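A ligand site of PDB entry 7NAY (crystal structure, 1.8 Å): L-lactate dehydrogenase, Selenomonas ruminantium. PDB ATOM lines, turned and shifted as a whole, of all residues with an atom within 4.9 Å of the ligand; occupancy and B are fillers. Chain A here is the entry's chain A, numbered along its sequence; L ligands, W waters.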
ATOM      1  N   ILE A  10       4.383 -12.225  11.272  1.00  0.00           N
ATOM      2  CA  ILE A  10       3.261 -12.209  10.316  1.00  0.00           C
ATOM      3  C   ILE A  10       3.654 -11.297   9.170  1.00  0.00           C
ATOM      4  O   ILE A  10       3.955 -10.134   9.424  1.00  0.00           O
ATOM      5  CB  ILE A  10       1.939 -11.823  11.010  1.00  0.00           C
ATOM      6  CG1 ILE A  10       1.757 -12.673  12.273  1.00  0.00           C
ATOM      7  CG2 ILE A  10       0.794 -11.988  10.003  1.00  0.00           C
ATOM      8  CD1 ILE A  10       0.533 -12.371  13.070  1.00  0.00           C
ATOM      9  N   GLY A  11       3.638 -11.824   7.958  1.00  0.00           N
ATOM     10  CA  GLY A  11       4.183 -11.184   6.759  1.00  0.00           C
ATOM     11  C   GLY A  11       5.621 -11.635   6.599  1.00  0.00           C
ATOM     12  O   GLY A  11       6.434 -11.380   7.540  1.00  0.00           O
ATOM     13  N   ALA A  12       5.890 -12.406   5.552  1.00  0.00           N
ATOM     14  CA  ALA A  12       7.190 -13.063   5.313  1.00  0.00           C
ATOM     15  C   ALA A  12       7.837 -12.461   4.057  1.00  0.00           C
ATOM     16  O   ALA A  12       8.490 -13.199   3.313  1.00  0.00           O
ATOM     17  CB  ALA A  12       6.942 -14.542   5.166  1.00  0.00           C
ATOM     18  N   SER A  13       7.582 -11.191   3.768  1.00  0.00           N
ATOM     19  CA  SER A  13       8.207 -10.514   2.608  1.00  0.00           C
ATOM     20  C   SER A  13       9.495  -9.813   3.093  1.00  0.00           C
ATOM     21  O   SER A  13      10.112 -10.272   4.062  1.00  0.00           O
ATOM     22  CB  SER A  13       7.215  -9.561   1.949  1.00  0.00           C
ATOM     23  OG  SER A  13       7.724  -8.988   0.772  1.00  0.00           O
ATOM     24  N   ASN A  14       9.842  -8.695   2.494  1.00  0.00           N
ATOM     25  CA  ASN A  14      11.145  -8.039   2.739  1.00  0.00           C
ATOM     26  C   ASN A  14      11.329  -7.740   4.237  1.00  0.00           C
ATOM     27  O   ASN A  14      12.398  -8.006   4.806  1.00  0.00           O
ATOM     28  CB  ASN A  14      11.242  -6.834   1.809  1.00  0.00           C
ATOM     29  CG  ASN A  14      11.408  -7.268   0.359  1.00  0.00           C
ATOM     30  OD1 ASN A  14      12.182  -8.178   0.046  1.00  0.00           O
ATOM     31  ND2 ASN A  14      10.697  -6.623  -0.509  1.00  0.00           N
ATOM     32  N   VAL A  15      10.320  -7.180   4.873  1.00  0.00           N
ATOM     33  CA  VAL A  15      10.435  -6.721   6.285  1.00  0.00           C
ATOM     34  C   VAL A  15      10.397  -7.924   7.214  1.00  0.00           C
ATOM     35  O   VAL A  15      11.298  -8.060   8.062  1.00  0.00           O
ATOM     36  CB  VAL A  15       9.354  -5.697   6.615  1.00  0.00           C
ATOM     37  CG1 VAL A  15       9.358  -5.373   8.086  1.00  0.00           C
ATOM     38  CG2 VAL A  15       9.513  -4.466   5.748  1.00  0.00           C
ATOM     39  N   GLY A  16       9.398  -8.789   7.058  1.00  0.00           N
ATOM     40  CA  GLY A  16       9.248  -9.949   7.944  1.00  0.00           C
ATOM     41  C   GLY A  16      10.447 -10.852   7.904  1.00  0.00           C
ATOM     42  O   GLY A  16      10.852 -11.380   8.967  1.00  0.00           O
ATOM     43  N   ILE A  35       4.159 -16.502   9.106  1.00  0.00           N
ATOM     44  CA  ILE A  35       2.741 -16.537   8.642  1.00  0.00           C
ATOM     45  C   ILE A  35       2.629 -15.547   7.499  1.00  0.00           C
ATOM     46  O   ILE A  35       3.033 -14.378   7.619  1.00  0.00           O
ATOM     47  CB  ILE A  35       1.755 -16.214   9.795  1.00  0.00           C
ATOM     48  CG1 ILE A  35       1.837 -17.257  10.913  1.00  0.00           C
ATOM     49  CG2 ILE A  35       0.365 -16.032   9.219  1.00  0.00           C
ATOM     50  CD1 ILE A  35       1.029 -16.942  12.145  1.00  0.00           C
ATOM     51  N   ASP A  36       2.049 -16.005   6.395  1.00  0.00           N
ATOM     52  CA  ASP A  36       1.742 -15.129   5.258  1.00  0.00           C
ATOM     53  C   ASP A  36       0.561 -15.738   4.485  1.00  0.00           C
ATOM     54  O   ASP A  36       0.522 -16.965   4.380  1.00  0.00           O
ATOM     55  CB  ASP A  36       2.963 -14.938   4.364  1.00  0.00           C
ATOM     56  CG  ASP A  36       2.918 -13.671   3.520  1.00  0.00           C
ATOM     57  OD1 ASP A  36       2.086 -13.619   2.570  1.00  0.00           O
ATOM     58  OD2 ASP A  36       3.717 -12.750   3.784  1.00  0.00           O
ATOM     59  N   LEU A  37      -0.318 -14.891   3.941  1.00  0.00           N
ATOM     60  CA  LEU A  37      -1.306 -15.311   2.903  1.00  0.00           C
ATOM     61  C   LEU A  37      -0.586 -16.097   1.814  1.00  0.00           C
ATOM     62  O   LEU A  37      -1.151 -17.064   1.317  1.00  0.00           O
ATOM     63  CB  LEU A  37      -1.974 -14.093   2.243  1.00  0.00           C
ATOM     64  CG  LEU A  37      -2.841 -13.229   3.138  1.00  0.00           C
ATOM     65  CD1 LEU A  37      -3.482 -12.124   2.301  1.00  0.00           C
ATOM     66  CD2 LEU A  37      -3.883 -14.059   3.877  1.00  0.00           C
ATOM     67  N   ASN A  38       0.600 -15.651   1.410  1.00  0.00           N
ATOM     68  CA  ASN A  38       1.433 -16.410   0.458  1.00  0.00           C
ATOM     69  C   ASN A  38       2.234 -17.447   1.279  1.00  0.00           C
ATOM     70  O   ASN A  38       3.369 -17.118   1.703  1.00  0.00           O
ATOM     71  CB  ASN A  38       2.350 -15.487  -0.320  1.00  0.00           C
ATOM     72  CG  ASN A  38       3.115 -16.209  -1.414  1.00  0.00           C
ATOM     73  OD1 ASN A  38       3.320 -17.420  -1.369  1.00  0.00           O
ATOM     74  ND2 ASN A  38       3.564 -15.443  -2.381  1.00  0.00           N
ATOM     75  N   TYR A  68      -2.068 -19.423  12.630  1.00  0.00           N
ATOM     76  CA  TYR A  68      -2.382 -18.686  13.877  1.00  0.00           C
ATOM     77  C   TYR A  68      -2.307 -19.598  15.091  1.00  0.00           C
ATOM     78  O   TYR A  68      -2.143 -19.053  16.192  1.00  0.00           O
ATOM     79  CB  TYR A  68      -3.679 -17.912  13.743  1.00  0.00           C
ATOM     80  CG  TYR A  68      -3.472 -16.666  12.930  1.00  0.00           C
ATOM     81  CD1 TYR A  68      -2.925 -15.534  13.501  1.00  0.00           C
ATOM     82  CD2 TYR A  68      -3.682 -16.667  11.556  1.00  0.00           C
ATOM     83  CE1 TYR A  68      -2.719 -14.381  12.757  1.00  0.00           C
ATOM     84  CE2 TYR A  68      -3.475 -15.541  10.795  1.00  0.00           C
ATOM     85  CZ  TYR A  68      -2.937 -14.408  11.395  1.00  0.00           C
ATOM     86  OH  TYR A  68      -2.690 -13.295  10.632  1.00  0.00           O
ATOM     87  N   THR A  80       4.139  -7.547  10.321  1.00  0.00           N
ATOM     88  CA  THR A  80       4.751  -6.872   9.158  1.00  0.00           C
ATOM     89  C   THR A  80       3.870  -7.011   7.910  1.00  0.00           C
ATOM     90  O   THR A  80       4.333  -6.611   6.864  1.00  0.00           O
ATOM     91  CB  THR A  80       6.161  -7.409   8.871  1.00  0.00           C
ATOM     92  OG1 THR A  80       6.064  -8.606   8.097  1.00  0.00           O
ATOM     93  CG2 THR A  80       6.975  -7.604  10.128  1.00  0.00           C
ATOM     94  N   ALA A  81       2.647  -7.522   8.031  1.00  0.00           N
ATOM     95  CA  ALA A  81       1.785  -7.865   6.882  1.00  0.00           C
ATOM     96  C   ALA A  81       1.257  -6.568   6.267  1.00  0.00           C
ATOM     97  O   ALA A  81       0.990  -5.581   7.004  1.00  0.00           O
ATOM     98  CB  ALA A  81       0.656  -8.745   7.323  1.00  0.00           C
ATOM     99  N   GLY A  82       1.091  -6.589   4.957  1.00  0.00           N
ATOM    100  CA  GLY A  82       0.434  -5.481   4.248  1.00  0.00           C
ATOM    101  C   GLY A  82       1.429  -4.750   3.380  1.00  0.00           C
ATOM    102  O   GLY A  82       2.636  -4.796   3.605  1.00  0.00           O
ATOM    103  N   PRO A  83       0.928  -4.048   2.344  1.00  0.00           N
ATOM    104  CA  PRO A  83       1.811  -3.382   1.404  1.00  0.00           C
ATOM    105  C   PRO A  83       2.495  -2.142   1.991  1.00  0.00           C
ATOM    106  O   PRO A  83       2.034  -1.576   2.992  1.00  0.00           O
ATOM    107  CB  PRO A  83       0.865  -3.025   0.229  1.00  0.00           C
ATOM    108  CG  PRO A  83      -0.517  -2.972   0.859  1.00  0.00           C
ATOM    109  CD  PRO A  83      -0.492  -4.015   1.940  1.00  0.00           C
ATOM    110  N   SER A  84       3.595  -1.784   1.353  1.00  0.00           N
ATOM    111  CA  SER A  84       4.295  -0.503   1.582  1.00  0.00           C
ATOM    112  C   SER A  84       3.945   0.513   0.481  1.00  0.00           C
ATOM    113  O   SER A  84       3.230   0.183  -0.460  1.00  0.00           O
ATOM    114  CB  SER A  84       5.790  -0.660   1.695  1.00  0.00           C
ATOM    115  OG  SER A  84       6.271   0.415   2.498  1.00  0.00           O
ATOM    116  N   ILE A  85       4.433   1.727   0.652  1.00  0.00           N
ATOM    117  CA  ILE A  85       4.504   2.727  -0.436  1.00  0.00           C
ATOM    118  C   ILE A  85       5.626   2.272  -1.362  1.00  0.00           C
ATOM    119  O   ILE A  85       6.636   1.653  -0.932  1.00  0.00           O
ATOM    120  CB  ILE A  85       4.660   4.148   0.113  1.00  0.00           C
ATOM    121  CG1 ILE A  85       5.940   4.332   0.922  1.00  0.00           C
ATOM    122  CG2 ILE A  85       3.413   4.579   0.886  1.00  0.00           C
ATOM    123  CD1 ILE A  85       6.076   5.709   1.535  1.00  0.00           C
ATOM    124  N   LEU A  96      -1.662   4.491   3.147  1.00  0.00           N
ATOM    125  CA  LEU A  96      -1.868   3.046   3.358  1.00  0.00           C
ATOM    126  C   LEU A  96      -2.952   2.816   4.410  1.00  0.00           C
ATOM    127  O   LEU A  96      -3.283   1.625   4.644  1.00  0.00           O
ATOM    128  CB  LEU A  96      -0.551   2.403   3.786  1.00  0.00           C
ATOM    129  CG  LEU A  96       0.574   2.463   2.764  1.00  0.00           C
ATOM    130  CD1 LEU A  96       1.886   2.034   3.407  1.00  0.00           C
ATOM    131  CD2 LEU A  96       0.277   1.578   1.572  1.00  0.00           C
ATOM    132  N   ASN A 100      -4.524  -0.935   5.035  1.00  0.00           N
ATOM    133  CA  ASN A 100      -3.721  -1.686   6.044  1.00  0.00           C
ATOM    134  C   ASN A 100      -4.469  -1.752   7.354  1.00  0.00           C
ATOM    135  O   ASN A 100      -4.190  -2.695   8.072  1.00  0.00           O
ATOM    136  CB  ASN A 100      -2.297  -1.156   6.146  1.00  0.00           C
ATOM    137  CG  ASN A 100      -1.520  -1.546   4.898  1.00  0.00           C
ATOM    138  OD1 ASN A 100      -2.086  -2.025   3.912  1.00  0.00           O
ATOM    139  ND2 ASN A 100      -0.239  -1.285   4.914  1.00  0.00           N
ATOM    140  N   ILE A 103      -6.356  -4.972   7.040  1.00  0.00           N
ATOM    141  CA  ILE A 103      -5.435  -6.145   7.233  1.00  0.00           C
ATOM    142  C   ILE A 103      -5.144  -6.312   8.732  1.00  0.00           C
ATOM    143  O   ILE A 103      -5.240  -7.424   9.226  1.00  0.00           O
ATOM    144  CB  ILE A 103      -4.149  -5.970   6.404  1.00  0.00           C
ATOM    145  CG1 ILE A 103      -4.462  -5.872   4.907  1.00  0.00           C
ATOM    146  CG2 ILE A 103      -3.147  -7.073   6.702  1.00  0.00           C
ATOM    147  CD1 ILE A 103      -3.294  -5.462   4.058  1.00  0.00           C
ATOM    148  N   SER A 106      -8.019  -7.860  10.524  1.00  0.00           N
ATOM    149  CA  SER A 106      -8.106  -9.293  10.179  1.00  0.00           C
ATOM    150  C   SER A 106      -7.032 -10.066  10.971  1.00  0.00           C
ATOM    151  O   SER A 106      -7.324 -11.065  11.638  1.00  0.00           O
ATOM    152  CB  SER A 106      -7.972  -9.422   8.715  1.00  0.00           C
ATOM    153  OG  SER A 106      -7.936 -10.770   8.344  1.00  0.00           O
ATOM    154  N   VAL A 107      -5.782  -9.577  10.948  1.00  0.00           N
ATOM    155  CA  VAL A 107      -4.645 -10.285  11.593  1.00  0.00           C
ATOM    156  C   VAL A 107      -4.850 -10.266  13.095  1.00  0.00           C
ATOM    157  O   VAL A 107      -4.703 -11.311  13.747  1.00  0.00           O
ATOM    158  CB  VAL A 107      -3.316  -9.608  11.186  1.00  0.00           C
ATOM    159  CG1 VAL A 107      -2.176 -10.073  12.059  1.00  0.00           C
ATOM    160  CG2 VAL A 107      -2.988  -9.791   9.714  1.00  0.00           C
ATOM    161  N   ILE A 123       4.800  -3.209  13.141  1.00  0.00           N
ATOM    162  CA  ILE A 123       5.739  -2.604  12.156  1.00  0.00           C
ATOM    163  C   ILE A 123       4.915  -2.116  10.940  1.00  0.00           C
ATOM    164  O   ILE A 123       5.241  -1.083  10.400  1.00  0.00           O
ATOM    165  CB  ILE A 123       6.812  -3.629  11.748  1.00  0.00           C
ATOM    166  CG1 ILE A 123       7.724  -3.975  12.933  1.00  0.00           C
ATOM    167  CG2 ILE A 123       7.601  -3.173  10.546  1.00  0.00           C
ATOM    168  CD1 ILE A 123       8.899  -4.844  12.570  1.00  0.00           C
ATOM    169  N   THR A 124       3.871  -2.868  10.581  1.00  0.00           N
ATOM    170  CA  THR A 124       3.019  -2.518   9.420  1.00  0.00           C
ATOM    171  C   THR A 124       2.672  -1.026   9.365  1.00  0.00           C
ATOM    172  O   THR A 124       2.279  -0.476  10.393  1.00  0.00           O
ATOM    173  CB  THR A 124       1.736  -3.355   9.418  1.00  0.00           C
ATOM    174  OG1 THR A 124       2.089  -4.721   9.217  1.00  0.00           O
ATOM    175  CG2 THR A 124       0.732  -2.890   8.379  1.00  0.00           C
ATOM    176  N   ASN A 125       2.802  -0.433   8.186  1.00  0.00           N
ATOM    177  CA  ASN A 125       2.458   0.995   7.989  1.00  0.00           C
ATOM    178  C   ASN A 125       0.977   1.174   7.657  1.00  0.00           C
ATOM    179  O   ASN A 125       0.310   0.242   7.193  1.00  0.00           O
ATOM    180  CB  ASN A 125       3.310   1.603   6.892  1.00  0.00           C
ATOM    181  CG  ASN A 125       4.562   2.208   7.467  1.00  0.00           C
ATOM    182  OD1 ASN A 125       4.482   2.937   8.462  1.00  0.00           O
ATOM    183  ND2 ASN A 125       5.682   1.965   6.802  1.00  0.00           N
ATOM    184  N   LEU A 127       2.447   3.112  10.587  1.00  0.00           N
ATOM    185  CA  LEU A 127       2.798   2.473  11.890  1.00  0.00           C
ATOM    186  C   LEU A 127       1.873   2.939  13.029  1.00  0.00           C
ATOM    187  O   LEU A 127       1.355   2.064  13.736  1.00  0.00           O
ATOM    188  CB  LEU A 127       4.264   2.853  12.144  1.00  0.00           C
ATOM    189  CG  LEU A 127       4.958   2.237  13.347  1.00  0.00           C
ATOM    190  CD1 LEU A 127       4.577   2.926  14.639  1.00  0.00           C
ATOM    191  CD2 LEU A 127       4.712   0.744  13.433  1.00  0.00           C
ATOM    192  N   THR A 148       7.143   0.044  16.637  1.00  0.00           N
ATOM    193  CA  THR A 148       8.574   0.446  16.561  1.00  0.00           C
ATOM    194  C   THR A 148       8.695   1.970  16.462  1.00  0.00           C
ATOM    195  O   THR A 148       9.600   2.513  17.085  1.00  0.00           O
ATOM    196  CB  THR A 148       9.253  -0.288  15.411  1.00  0.00           C
ATOM    197  OG1 THR A 148       8.446  -0.065  14.249  1.00  0.00           O
ATOM    198  CG2 THR A 148       9.323  -1.766  15.709  1.00  0.00           C
ATOM    199  N   LEU A 152      13.230   4.038  14.568  1.00  0.00           N
ATOM    200  CA  LEU A 152      13.976   3.989  13.287  1.00  0.00           C
ATOM    201  C   LEU A 152      14.410   5.424  12.899  1.00  0.00           C
ATOM    202  O   LEU A 152      15.589   5.610  12.552  1.00  0.00           O
ATOM    203  CB  LEU A 152      13.130   3.283  12.235  1.00  0.00           C
ATOM    204  CG  LEU A 152      13.778   3.029  10.863  1.00  0.00           C
ATOM    205  CD1 LEU A 152      15.178   2.457  10.990  1.00  0.00           C
ATOM    206  CD2 LEU A 152      12.910   2.096  10.035  1.00  0.00           C
ATOM    207  N   HIS A 180       5.768   8.119  12.847  1.00  0.00           N
ATOM    208  CA  HIS A 180       6.708   7.446  11.926  1.00  0.00           C
ATOM    209  C   HIS A 180       6.273   7.854  10.519  1.00  0.00           C
ATOM    210  O   HIS A 180       5.473   7.137   9.909  1.00  0.00           O
ATOM    211  CB  HIS A 180       6.774   5.925  12.148  1.00  0.00           C
ATOM    212  CG  HIS A 180       7.642   5.274  11.133  1.00  0.00           C
ATOM    213  ND1 HIS A 180       9.028   5.386  11.156  1.00  0.00           N
ATOM    214  CD2 HIS A 180       7.324   4.532  10.059  1.00  0.00           C
ATOM    215  CE1 HIS A 180       9.509   4.702  10.135  1.00  0.00           C
ATOM    216  NE2 HIS A 180       8.484   4.192   9.425  1.00  0.00           N
ATOM    217  N   PHE A 233      12.428  -0.616  -1.363  1.00  0.00           N
ATOM    218  CA  PHE A 233      11.787  -0.905  -0.048  1.00  0.00           C
ATOM    219  C   PHE A 233      12.870  -0.675   1.019  1.00  0.00           C
ATOM    220  O   PHE A 233      14.026  -0.383   0.656  1.00  0.00           O
ATOM    221  CB  PHE A 233      11.256  -2.340  -0.027  1.00  0.00           C
ATOM    222  CG  PHE A 233      12.306  -3.379  -0.293  1.00  0.00           C
ATOM    223  CD1 PHE A 233      12.583  -3.790  -1.594  1.00  0.00           C
ATOM    224  CD2 PHE A 233      13.051  -3.918   0.750  1.00  0.00           C
ATOM    225  CE1 PHE A 233      13.558  -4.754  -1.838  1.00  0.00           C
ATOM    226  CE2 PHE A 233      14.027  -4.882   0.506  1.00  0.00           C
ATOM    227  CZ  PHE A 233      14.300  -5.274  -0.790  1.00  0.00           C
ATOM    228  N   THR A 234      12.485  -0.775   2.292  1.00  0.00           N
ATOM    229  CA  THR A 234      13.480  -0.751   3.391  1.00  0.00           C
ATOM    230  C   THR A 234      13.219  -1.992   4.261  1.00  0.00           C
ATOM    231  O   THR A 234      12.078  -2.458   4.279  1.00  0.00           O
ATOM    232  CB  THR A 234      13.360   0.463   4.324  1.00  0.00           C
ATOM    233  OG1 THR A 234      12.348   0.226   5.307  1.00  0.00           O
ATOM    234  CG2 THR A 234      13.120   1.760   3.580  1.00  0.00           C
ATOM    235  N   ILE A 238      14.691  -1.263  10.070  1.00  0.00           N
ATOM    236  CA  ILE A 238      13.473  -1.666  10.856  1.00  0.00           C
ATOM    237  C   ILE A 238      13.694  -3.034  11.541  1.00  0.00           C
ATOM    238  O   ILE A 238      13.229  -3.164  12.715  1.00  0.00           O
ATOM    239  CB  ILE A 238      12.180  -1.637  10.031  1.00  0.00           C
ATOM    240  CG1 ILE A 238      10.975  -1.949  10.918  1.00  0.00           C
ATOM    241  CG2 ILE A 238      12.233  -2.535   8.834  1.00  0.00           C
ATOM    242  CD1 ILE A 238      10.773  -1.004  12.070  1.00  0.00           C
HETATM  243  P1  LIG L   1       5.387  -6.262   1.010  1.00  0.00           P
HETATM  244  O1  LIG L   1       4.219  -5.660   0.307  1.00  0.00           O
HETATM  245  O2  LIG L   1       6.587  -6.609   0.208  1.00  0.00           O
HETATM  246  O3  LIG L   1       4.903  -7.572   1.780  1.00  0.00           O
HETATM  247  C1  LIG L   1       3.748  -7.587   2.626  1.00  0.00           C
HETATM  248  C2  LIG L   1       3.430  -9.026   2.919  1.00  0.00           C
HETATM  249  O4  LIG L   1       2.239  -9.115   3.739  1.00  0.00           O
HETATM  250  C3  LIG L   1       3.158  -9.905   1.688  1.00  0.00           C
HETATM  251  O5  LIG L   1       3.968 -11.077   1.725  1.00  0.00           O
HETATM  252  C4  LIG L   1       1.667 -10.251   1.822  1.00  0.00           C
HETATM  253  O6  LIG L   1       1.326 -11.491   1.250  1.00  0.00           O
HETATM  254  C5  LIG L   1       1.513 -10.233   3.327  1.00  0.00           C
HETATM  255  N1  LIG L   1       0.137 -10.089   3.790  1.00  0.00           N
HETATM  256  C6  LIG L   1      -0.802  -9.209   3.311  1.00  0.00           C
HETATM  257  N2  LIG L   1      -1.948  -9.305   3.926  1.00  0.00           N
HETATM  258  C7  LIG L   1      -1.752 -10.315   4.861  1.00  0.00           C
HETATM  259  C8  LIG L   1      -2.606 -10.896   5.822  1.00  0.00           C
HETATM  260  N3  LIG L   1      -3.871 -10.523   6.005  1.00  0.00           N
HETATM  261  N4  LIG L   1      -2.106 -11.881   6.587  1.00  0.00           N
HETATM  262  C9  LIG L   1      -0.833 -12.251   6.399  1.00  0.00           C
HETATM  263  N5  LIG L   1       0.062 -11.783   5.526  1.00  0.00           N
HETATM  264  C10 LIG L   1      -0.472 -10.809   4.779  1.00  0.00           C
HETATM  265  O7  LIG L   1       5.813  -5.299   2.207  1.00  0.00           O
HETATM  266  P2  LIG L   1       7.177  -5.115   3.036  1.00  0.00           P
HETATM  267  O8  LIG L   1       8.180  -4.370   2.236  1.00  0.00           O
HETATM  268  O9  LIG L   1       7.554  -6.447   3.595  1.00  0.00           O
HETATM  269  O10 LIG L   1       6.679  -4.173   4.215  1.00  0.00           O
HETATM  270  C11 LIG L   1       5.706  -4.717   5.112  1.00  0.00           C
HETATM  271  C12 LIG L   1       5.069  -3.596   5.897  1.00  0.00           C
HETATM  272  O11 LIG L   1       6.055  -3.023   6.771  1.00  0.00           O
HETATM  273  C13 LIG L   1       4.532  -2.426   5.054  1.00  0.00           C
HETATM  274  O12 LIG L   1       3.302  -1.962   5.574  1.00  0.00           O
HETATM  275  C14 LIG L   1       5.648  -1.394   5.225  1.00  0.00           C
HETATM  276  O13 LIG L   1       5.262  -0.065   4.931  1.00  0.00           O
HETATM  277  C15 LIG L   1       5.977  -1.618   6.691  1.00  0.00           C
HETATM  278  N6  LIG L   1       7.291  -1.034   7.083  1.00  0.00           N
HETATM  279  C16 LIG L   1       7.394  -0.401   8.282  1.00  0.00           C
HETATM  280  C17 LIG L   1       8.586   0.173   8.664  1.00  0.00           C
HETATM  281  C18 LIG L   1       8.615   0.918   9.974  1.00  0.00           C
HETATM  282  O14 LIG L   1       9.600   1.570  10.270  1.00  0.00           O
HETATM  283  N7  LIG L   1       7.561   0.801  10.765  1.00  0.00           N
HETATM  284  C19 LIG L   1       9.692   0.033   7.847  1.00  0.00           C
HETATM  285  C20 LIG L   1       9.597  -0.694   6.687  1.00  0.00           C
HETATM  286  C21 LIG L   1       8.365  -1.168   6.298  1.00  0.00           C
HETATM  287  O   HOH W   1       4.770 -12.175  -0.778  1.00  0.00           O
HETATM  288  O   HOH W   2      -5.974  -9.228   4.294  1.00  0.00           O
HETATM  289  O   HOH W   3       9.563  -2.152   3.264  1.00  0.00           O
HETATM  290  O   HOH W   4      -0.079  -7.318   0.667  1.00  0.00           O
HETATM  291  O   HOH W   5       7.278  -2.930  -0.411  1.00  0.00           O
HETATM  292  O   HOH W   6      -4.107  -8.582   2.287  1.00  0.00           O
HETATM  293  O   HOH W   7       6.952  -8.603   5.247  1.00  0.00           O
HETATM  294  O   HOH W   8       4.694  -3.291  -0.878  1.00  0.00           O
HETATM  295  O   HOH W   9       8.898  -5.084   0.001  1.00  0.00           O
HETATM  296  O   HOH W  10       9.135   2.123  12.880  1.00  0.00           O
HETATM  297  O   HOH W  11       6.316  -7.184  -2.619  1.00  0.00           O
HETATM  298  O   HOH W  12       2.181  -6.780  -0.722  1.00  0.00           O
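OD1 of Asp 36 lies within hydrogen-bond range of O6 of the ligand (2.6 Å).
The side-chain hydroxyl (OG) of Ser 84 sits at hydrogen-bond distance from an oxygen (O13) of the ligand (2.7 Å).
O2 of the ligand lies within hydrogen-bond range of OG of Ser 13, at 2.7 Å.
An oxygen (O12) of the ligand lies within hydrogen-bond range of the backbone NH (N) of Asn 125, 3.1 Å away.
The side-chain amide nitrogen (ND2) of Asn 125 lies within hydrogen-bond range of an oxygen (O13) of the ligand (2.8 Å).
The backbone carbonyl oxygen of Pro 83 lies within hydrogen-bond range of an oxygen (O12) of the ligand.
NE2 of His 180 lies within hydrogen-bond range of O14 of the ligand (3.0 Å).
O of Ile 123 lies within hydrogen-bond range of N7 of the ligand, at 3.0 Å.
N of Gly 82 is in hydrogen-bond range of O4 of the ligand, 3.0 Å away.
O9 of the ligand sits at hydrogen-bond distance from N of Val 15, 3.1 Å away.
An oxygen (O9) of the ligand is in hydrogen-bond range of the backbone NH (N) of Asn 14 (3.4 Å).
Merely in contact with the ligand: Ile 10, Leu 37, Thr 80, Ala 81, Asn 100, Ile 103, Val 107, Thr 124, Leu 127, Thr 148, Leu 152, Thr 234 and Ile 238.
Hydrophobic or aromatic side chains that line the ligand: Ile 10, Val 15, Leu 37, Ala 81, Ile 103, Val 107, Ile 123, Leu 127, Leu 152, His 180 and Ile 238.
Within 4 Å of the ligand: Ile 10, Ser 13, Asn 14, Val 15, Asp 36, Leu 37, Thr 80, Ala 81, Gly 82, Pro 83, Ser 84, Asn 100, Ile 103, Val 107, Ile 123, Thr 124, Asn 125, Leu 127, Thr 148, Leu 152, His 180, Thr 234 and Ile 238.
Water W9 lies within hydrogen-bond range of ND2 of Asn 14 (2.4 Å) and O8 of the ligand (2.5 Å).
Water W8 lies within hydrogen-bond range of an oxygen (O1) of the ligand (2.7 Å) and the backbone NH (N) of Ser 84 (2.9 Å).
Water W10 bridges the side-chain hydroxyl (OG1) of Thr 148 and an oxygen (O14) of the ligand.
Water W7 lies within hydrogen-bond range of O9 of the ligand (2.8 Å), OG1 of Thr 80 (3.0 Å), N of Ser 13 (3.0 Å) and N of Gly 16 (3.0 Å).
Water W3 bridges O of Thr 234 and O8 of the ligand.
The backbone NH (N) of Asn 38 lies within hydrogen-bond range of the side-chain carboxylate (OD1) of Asp 36, 2.8 Å away.
The side-chain carboxylate (OD2) of Asp 36 is in hydrogen-bond range of the backbone NH (N) of Ala 12 (2.8 Å).
The backbone carbonyl oxygen of Asn 125 sits at hydrogen-bond distance from the side-chain amide nitrogen of Asn 100, at 2.8 Å.
The backbone NH (N) of Leu 127 lies within hydrogen-bond range of the side-chain amide oxygen (OD1) of Asn 125 (2.9 Å).
The side-chain amide nitrogen (ND2) of Asn 100 is in hydrogen-bond range of the backbone carbonyl oxygen (O) of Pro 83.
The backbone carbonyl oxygen (O) of Gly 11 sits at hydrogen-bond distance from the side-chain hydroxyl (OG1) of Thr 80 (2.9 Å).
N of Gly 16 sits close to OG1 of Thr 80, at 3.5 Å.
OG1 of Thr 124 is in hydrogen-bond range of O of Ala 81 (2.6 Å).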
